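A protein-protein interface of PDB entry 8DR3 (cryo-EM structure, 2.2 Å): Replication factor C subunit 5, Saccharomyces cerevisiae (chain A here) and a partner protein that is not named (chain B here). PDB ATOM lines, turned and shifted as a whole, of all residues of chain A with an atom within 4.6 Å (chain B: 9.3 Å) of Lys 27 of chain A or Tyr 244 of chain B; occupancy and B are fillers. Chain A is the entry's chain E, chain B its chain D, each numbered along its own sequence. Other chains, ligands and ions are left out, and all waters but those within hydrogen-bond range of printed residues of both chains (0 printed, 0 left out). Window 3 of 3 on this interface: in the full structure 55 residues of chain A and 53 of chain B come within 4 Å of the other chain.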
ATOM      1  N   LEU A  13      31.294 -17.022   3.394  1.00  0.00           N
ATOM      2  CA  LEU A  13      30.442 -17.651   2.391  1.00  0.00           C
ATOM      3  C   LEU A  13      30.725 -17.093   1.003  1.00  0.00           C
ATOM      4  O   LEU A  13      30.759 -17.840   0.019  1.00  0.00           O
ATOM      5  CB  LEU A  13      28.970 -17.460   2.756  1.00  0.00           C
ATOM      6  CG  LEU A  13      28.408 -18.381   3.843  1.00  0.00           C
ATOM      7  CD1 LEU A  13      26.971 -18.001   4.168  1.00  0.00           C
ATOM      8  CD2 LEU A  13      28.491 -19.842   3.428  1.00  0.00           C
ATOM      9  N   ASN A  14      30.933 -15.778   0.904  1.00  0.00           N
ATOM     10  CA  ASN A  14      31.218 -15.163  -0.386  1.00  0.00           C
ATOM     11  C   ASN A  14      32.561 -15.600  -0.955  1.00  0.00           C
ATOM     12  O   ASN A  14      32.797 -15.422  -2.154  1.00  0.00           O
ATOM     13  CB  ASN A  14      31.185 -13.639  -0.258  1.00  0.00           C
ATOM     14  CG  ASN A  14      29.787 -13.102  -0.033  1.00  0.00           C
ATOM     15  OD1 ASN A  14      29.514 -12.449   0.974  1.00  0.00           O
ATOM     16  ND2 ASN A  14      28.891 -13.372  -0.974  1.00  0.00           N
ATOM     17  N   THR A  23      26.171 -22.901  -1.690  1.00  0.00           N
ATOM     18  CA  THR A  23      26.432 -21.594  -1.094  1.00  0.00           C
ATOM     19  C   THR A  23      25.153 -20.774  -0.984  1.00  0.00           C
ATOM     20  O   THR A  23      24.903 -20.131   0.041  1.00  0.00           O
ATOM     21  CB  THR A  23      27.480 -20.843  -1.917  1.00  0.00           C
ATOM     22  OG1 THR A  23      28.693 -21.604  -1.965  1.00  0.00           O
ATOM     23  CG2 THR A  23      27.765 -19.476  -1.311  1.00  0.00           C
ATOM     24  N   ASN A  24      24.329 -20.785  -2.035  1.00  0.00           N
ATOM     25  CA  ASN A  24      23.062 -20.064  -1.986  1.00  0.00           C
ATOM     26  C   ASN A  24      22.143 -20.640  -0.917  1.00  0.00           C
ATOM     27  O   ASN A  24      21.460 -19.894  -0.204  1.00  0.00           O
ATOM     28  CB  ASN A  24      22.382 -20.101  -3.355  1.00  0.00           C
ATOM     29  CG  ASN A  24      23.192 -19.398  -4.427  1.00  0.00           C
ATOM     30  OD1 ASN A  24      23.935 -18.457  -4.144  1.00  0.00           O
ATOM     31  ND2 ASN A  24      23.053 -19.850  -5.667  1.00  0.00           N
ATOM     32  N   PHE A  25      22.103 -21.969  -0.795  1.00  0.00           N
ATOM     33  CA  PHE A  25      21.276 -22.588   0.238  1.00  0.00           C
ATOM     34  C   PHE A  25      21.750 -22.192   1.633  1.00  0.00           C
ATOM     35  O   PHE A  25      20.935 -21.908   2.520  1.00  0.00           O
ATOM     36  CB  PHE A  25      21.292 -24.107   0.076  1.00  0.00           C
ATOM     37  CG  PHE A  25      20.675 -24.844   1.226  1.00  0.00           C
ATOM     38  CD1 PHE A  25      19.299 -24.905   1.370  1.00  0.00           C
ATOM     39  CD2 PHE A  25      21.469 -25.476   2.167  1.00  0.00           C
ATOM     40  CE1 PHE A  25      18.729 -25.583   2.428  1.00  0.00           C
ATOM     41  CE2 PHE A  25      20.903 -26.155   3.227  1.00  0.00           C
ATOM     42  CZ  PHE A  25      19.531 -26.209   3.358  1.00  0.00           C
ATOM     43  N   LEU A  26      23.068 -22.167   1.847  1.00  0.00           N
ATOM     44  CA  LEU A  26      23.598 -21.761   3.144  1.00  0.00           C
ATOM     45  C   LEU A  26      23.279 -20.298   3.432  1.00  0.00           C
ATOM     46  O   LEU A  26      22.956 -19.936   4.571  1.00  0.00           O
ATOM     47  CB  LEU A  26      25.108 -22.002   3.192  1.00  0.00           C
ATOM     48  CG  LEU A  26      25.559 -23.466   3.183  1.00  0.00           C
ATOM     49  CD1 LEU A  26      27.077 -23.555   3.169  1.00  0.00           C
ATOM     50  CD2 LEU A  26      24.991 -24.224   4.374  1.00  0.00           C
ATOM     51  N   LYS A  27      23.368 -19.440   2.413  1.00  0.00           N
ATOM     52  CA  LYS A  27      22.986 -18.043   2.593  1.00  0.00           C
ATOM     53  C   LYS A  27      21.515 -17.924   2.970  1.00  0.00           C
ATOM     54  O   LYS A  27      21.150 -17.131   3.847  1.00  0.00           O
ATOM     55  CB  LYS A  27      23.279 -17.252   1.317  1.00  0.00           C
ATOM     56  CG  LYS A  27      24.748 -16.930   1.112  1.00  0.00           C
ATOM     57  CD  LYS A  27      25.011 -16.403  -0.287  1.00  0.00           C
ATOM     58  CE  LYS A  27      26.443 -15.923  -0.439  1.00  0.00           C
ATOM     59  NZ  LYS A  27      26.754 -15.528  -1.841  1.00  0.00           N
ATOM     60  N   SER A  28      20.652 -18.705   2.315  1.00  0.00           N
ATOM     61  CA  SER A  28      19.235 -18.692   2.661  1.00  0.00           C
ATOM     62  C   SER A  28      19.021 -19.134   4.102  1.00  0.00           C
ATOM     63  O   SER A  28      18.196 -18.558   4.822  1.00  0.00           O
ATOM     64  CB  SER A  28      18.453 -19.590   1.703  1.00  0.00           C
ATOM     65  OG  SER A  28      18.430 -20.929   2.163  1.00  0.00           O
ATOM     66  N   LEU A  29      19.751 -20.161   4.540  1.00  0.00           N
ATOM     67  CA  LEU A  29      19.641 -20.602   5.927  1.00  0.00           C
ATOM     68  C   LEU A  29      20.079 -19.503   6.887  1.00  0.00           C
ATOM     69  O   LEU A  29      19.449 -19.289   7.929  1.00  0.00           O
ATOM     70  CB  LEU A  29      20.476 -21.863   6.150  1.00  0.00           C
ATOM     71  CG  LEU A  29      19.887 -23.196   5.682  1.00  0.00           C
ATOM     72  CD1 LEU A  29      20.853 -24.327   5.999  1.00  0.00           C
ATOM     73  CD2 LEU A  29      18.527 -23.459   6.311  1.00  0.00           C
ATOM     74  N   SER A  30      21.160 -18.798   6.553  1.00  0.00           N
ATOM     75  CA  SER A  30      21.688 -17.752   7.420  1.00  0.00           C
ATOM     76  C   SER A  30      20.909 -16.447   7.330  1.00  0.00           C
ATOM     77  O   SER A  30      21.167 -15.538   8.126  1.00  0.00           O
ATOM     78  CB  SER A  30      23.155 -17.484   7.080  1.00  0.00           C
ATOM     79  OG  SER A  30      23.297 -17.064   5.736  1.00  0.00           O
ATOM     80  N   ASP A  31      19.976 -16.325   6.384  1.00  0.00           N
ATOM     81  CA  ASP A  31      19.221 -15.083   6.251  1.00  0.00           C
ATOM     82  C   ASP A  31      18.437 -14.770   7.521  1.00  0.00           C
ATOM     83  O   ASP A  31      18.425 -13.624   7.986  1.00  0.00           O
ATOM     84  CB  ASP A  31      18.279 -15.173   5.051  1.00  0.00           C
ATOM     85  CG  ASP A  31      17.651 -13.840   4.702  1.00  0.00           C
ATOM     86  OD1 ASP A  31      18.374 -12.821   4.699  1.00  0.00           O
ATOM     87  OD2 ASP A  31      16.433 -13.810   4.430  1.00  0.00           O
ATOM     88  N   GLN B 236       9.978 -26.233   6.479  1.00  0.00           N
ATOM     89  CA  GLN B 236      10.660 -25.031   6.950  1.00  0.00           C
ATOM     90  C   GLN B 236      11.840 -24.682   6.052  1.00  0.00           C
ATOM     91  O   GLN B 236      12.067 -23.507   5.741  1.00  0.00           O
ATOM     92  CB  GLN B 236      11.124 -25.218   8.395  1.00  0.00           C
ATOM     93  CG  GLN B 236      11.686 -23.950   9.024  1.00  0.00           C
ATOM     94  CD  GLN B 236      12.056 -24.127  10.485  1.00  0.00           C
ATOM     95  OE1 GLN B 236      11.948 -25.219  11.040  1.00  0.00           O
ATOM     96  NE2 GLN B 236      12.501 -23.047  11.114  1.00  0.00           N
ATOM     97  N   SER B 237      12.607 -25.690   5.631  1.00  0.00           N
ATOM     98  CA  SER B 237      13.727 -25.434   4.727  1.00  0.00           C
ATOM     99  C   SER B 237      13.246 -24.843   3.407  1.00  0.00           C
ATOM    100  O   SER B 237      13.834 -23.882   2.893  1.00  0.00           O
ATOM    101  CB  SER B 237      14.504 -26.725   4.478  1.00  0.00           C
ATOM    102  OG  SER B 237      15.533 -26.891   5.434  1.00  0.00           O
ATOM    103  N   ALA B 238      12.178 -25.410   2.842  1.00  0.00           N
ATOM    104  CA  ALA B 238      11.647 -24.891   1.585  1.00  0.00           C
ATOM    105  C   ALA B 238      11.143 -23.462   1.750  1.00  0.00           C
ATOM    106  O   ALA B 238      11.348 -22.617   0.870  1.00  0.00           O
ATOM    107  CB  ALA B 238      10.530 -25.800   1.075  1.00  0.00           C
ATOM    108  N   SER B 239      10.475 -23.177   2.870  1.00  0.00           N
ATOM    109  CA  SER B 239       9.998 -21.822   3.121  1.00  0.00           C
ATOM    110  C   SER B 239      11.159 -20.844   3.231  1.00  0.00           C
ATOM    111  O   SER B 239      11.094 -19.729   2.699  1.00  0.00           O
ATOM    112  CB  SER B 239       9.152 -21.794   4.395  1.00  0.00           C
ATOM    113  OG  SER B 239       8.790 -20.469   4.737  1.00  0.00           O
ATOM    114  N   LYS B 240      12.228 -21.239   3.925  1.00  0.00           N
ATOM    115  CA  LYS B 240      13.400 -20.377   4.024  1.00  0.00           C
ATOM    116  C   LYS B 240      14.001 -20.114   2.650  1.00  0.00           C
ATOM    117  O   LYS B 240      14.371 -18.977   2.329  1.00  0.00           O
ATOM    118  CB  LYS B 240      14.441 -21.010   4.947  1.00  0.00           C
ATOM    119  CG  LYS B 240      14.203 -20.759   6.425  1.00  0.00           C
ATOM    120  CD  LYS B 240      15.501 -20.820   7.210  1.00  0.00           C
ATOM    121  CE  LYS B 240      15.253 -21.125   8.676  1.00  0.00           C
ATOM    122  NZ  LYS B 240      16.354 -20.622   9.541  1.00  0.00           N
ATOM    123  N   GLY B 241      14.106 -21.156   1.823  1.00  0.00           N
ATOM    124  CA  GLY B 241      14.633 -20.963   0.482  1.00  0.00           C
ATOM    125  C   GLY B 241      13.786 -20.007  -0.336  1.00  0.00           C
ATOM    126  O   GLY B 241      14.305 -19.107  -1.003  1.00  0.00           O
ATOM    127  N   ALA B 242      12.463 -20.186  -0.286  1.00  0.00           N
ATOM    128  CA  ALA B 242      11.571 -19.309  -1.038  1.00  0.00           C
ATOM    129  C   ALA B 242      11.678 -17.869  -0.552  1.00  0.00           C
ATOM    130  O   ALA B 242      11.722 -16.935  -1.361  1.00  0.00           O
ATOM    131  CB  ALA B 242      10.131 -19.804  -0.926  1.00  0.00           C
ATOM    132  N   GLN B 243      11.721 -17.667   0.766  1.00  0.00           N
ATOM    133  CA  GLN B 243      11.831 -16.314   1.300  1.00  0.00           C
ATOM    134  C   GLN B 243      13.143 -15.666   0.882  1.00  0.00           C
ATOM    135  O   GLN B 243      13.171 -14.484   0.518  1.00  0.00           O
ATOM    136  CB  GLN B 243      11.709 -16.338   2.825  1.00  0.00           C
ATOM    137  CG  GLN B 243      10.298 -16.572   3.367  1.00  0.00           C
ATOM    138  CD  GLN B 243       9.223 -15.833   2.588  1.00  0.00           C
ATOM    139  OE1 GLN B 243       8.595 -16.394   1.691  1.00  0.00           O
ATOM    140  NE2 GLN B 243       9.007 -14.569   2.931  1.00  0.00           N
ATOM    141  N   TYR B 244      14.243 -16.420   0.926  1.00  0.00           N
ATOM    142  CA  TYR B 244      15.525 -15.863   0.509  1.00  0.00           C
ATOM    143  C   TYR B 244      15.513 -15.508  -0.972  1.00  0.00           C
ATOM    144  O   TYR B 244      16.052 -14.471  -1.373  1.00  0.00           O
ATOM    145  CB  TYR B 244      16.654 -16.846   0.808  1.00  0.00           C
ATOM    146  CG  TYR B 244      18.006 -16.368   0.335  1.00  0.00           C
ATOM    147  CD1 TYR B 244      18.644 -15.304   0.959  1.00  0.00           C
ATOM    148  CD2 TYR B 244      18.643 -16.974  -0.737  1.00  0.00           C
ATOM    149  CE1 TYR B 244      19.879 -14.861   0.530  1.00  0.00           C
ATOM    150  CE2 TYR B 244      19.878 -16.538  -1.174  1.00  0.00           C
ATOM    151  CZ  TYR B 244      20.491 -15.481  -0.536  1.00  0.00           C
ATOM    152  OH  TYR B 244      21.722 -15.044  -0.968  1.00  0.00           O
ATOM    153  N   LEU B 245      14.907 -16.360  -1.803  1.00  0.00           N
ATOM    154  CA  LEU B 245      14.877 -16.089  -3.237  1.00  0.00           C
ATOM    155  C   LEU B 245      14.159 -14.776  -3.529  1.00  0.00           C
ATOM    156  O   LEU B 245      14.633 -13.960  -4.328  1.00  0.00           O
ATOM    157  CB  LEU B 245      14.206 -17.250  -3.973  1.00  0.00           C
ATOM    158  CG  LEU B 245      14.238 -17.226  -5.505  1.00  0.00           C
ATOM    159  CD1 LEU B 245      15.597 -16.793  -6.036  1.00  0.00           C
ATOM    160  CD2 LEU B 245      13.858 -18.590  -6.061  1.00  0.00           C
ATOM    161  N   GLY B 246      13.012 -14.556  -2.890  1.00  0.00           N
ATOM    162  CA  GLY B 246      12.283 -13.314  -3.029  1.00  0.00           C
ATOM    163  C   GLY B 246      11.472 -13.177  -4.297  1.00  0.00           C
ATOM    164  O   GLY B 246      10.868 -12.119  -4.511  1.00  0.00           O
ATOM    165  N   ASP B 247      11.433 -14.207  -5.144  1.00  0.00           N
ATOM    166  CA  ASP B 247      10.686 -14.116  -6.393  1.00  0.00           C
ATOM    167  C   ASP B 247       9.180 -14.165  -6.173  1.00  0.00           C
ATOM    168  O   ASP B 247       8.427 -13.681  -7.025  1.00  0.00           O
ATOM    169  CB  ASP B 247      11.106 -15.244  -7.336  1.00  0.00           C
ATOM    170  CG  ASP B 247      10.907 -14.887  -8.797  1.00  0.00           C
ATOM    171  OD1 ASP B 247      10.130 -13.952  -9.083  1.00  0.00           O
ATOM    172  OD2 ASP B 247      11.529 -15.543  -9.659  1.00  0.00           O
ATOM    173  N   GLY B 248       8.725 -14.733  -5.060  1.00  0.00           N
ATOM    174  CA  GLY B 248       7.310 -14.873  -4.796  1.00  0.00           C
ATOM    175  C   GLY B 248       6.649 -16.050  -5.478  1.00  0.00           C
ATOM    176  O   GLY B 248       5.435 -16.231  -5.321  1.00  0.00           O
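The side-chain amino group (NZ) of Lys 27 of chain A lies close to the side-chain amide nitrogen (ND2) of Asn 14 of chain A (3.2 Å).
The backbone carbonyl oxygen of Phe 25 of chain A is in hydrogen-bond range of the side-chain hydroxyl of Ser 28 of chain A, at 2.7 Å.
The backbone carbonyl oxygen of Lys 27 of chain A sits at hydrogen-bond distance from the side-chain hydroxyl of Ser 30 of chain A, 2.9 Å away.
Of the printed residues of chain B, Asn 24 of chain A touches Tyr 244.
Printed residues of chain B within 4 Å of Ser 28 of chain A: Tyr 244 (3.4 Å).
Of the printed residues of chain B, Leu 29 of chain A touches Lys 240 (3.7 Å).
No residue of chain B comes within 4 Å of Ser 30 of chain A.
Of the printed residues of chain A, Lys 240 of chain B touches Leu 29.
Gly 241 of chain B touches none of the printed residues of chain A.
Tyr 244 of chain B touches just these residues of chain A: Asn 24 (3.8 Å), Lys 27 (3.5 Å) and Ser 28 (3.4 Å).
Printed residues of chain B that touch a printed residue of chain A: Lys 240 and Tyr 244.
Hydrophobic or aromatic side chains of chain B within 4 Å of the printed part of chain A: Tyr 244.
Of the 11 printed residues of chain A, 4 touch a printed residue of chain B.
Among the printed residues, 4 pairs touch across the chains.
Among the printed residues, no Asp or Glu carboxylate lies within 4 Å of a Lys or Arg side-chain nitrogen of the other chain.
Among the printed residues, merely in contact across the chains: Asn 24 of chain A with Tyr 244 of chain B (3.8 Å), Lys 27 of chain A with Tyr 244 of chain B (3.5 Å), Ser 28 of chain A with Tyr 244 of chain B (3.4 Å) and Leu 29 of chain A with Lys 240 of chain B (3.7 Å).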
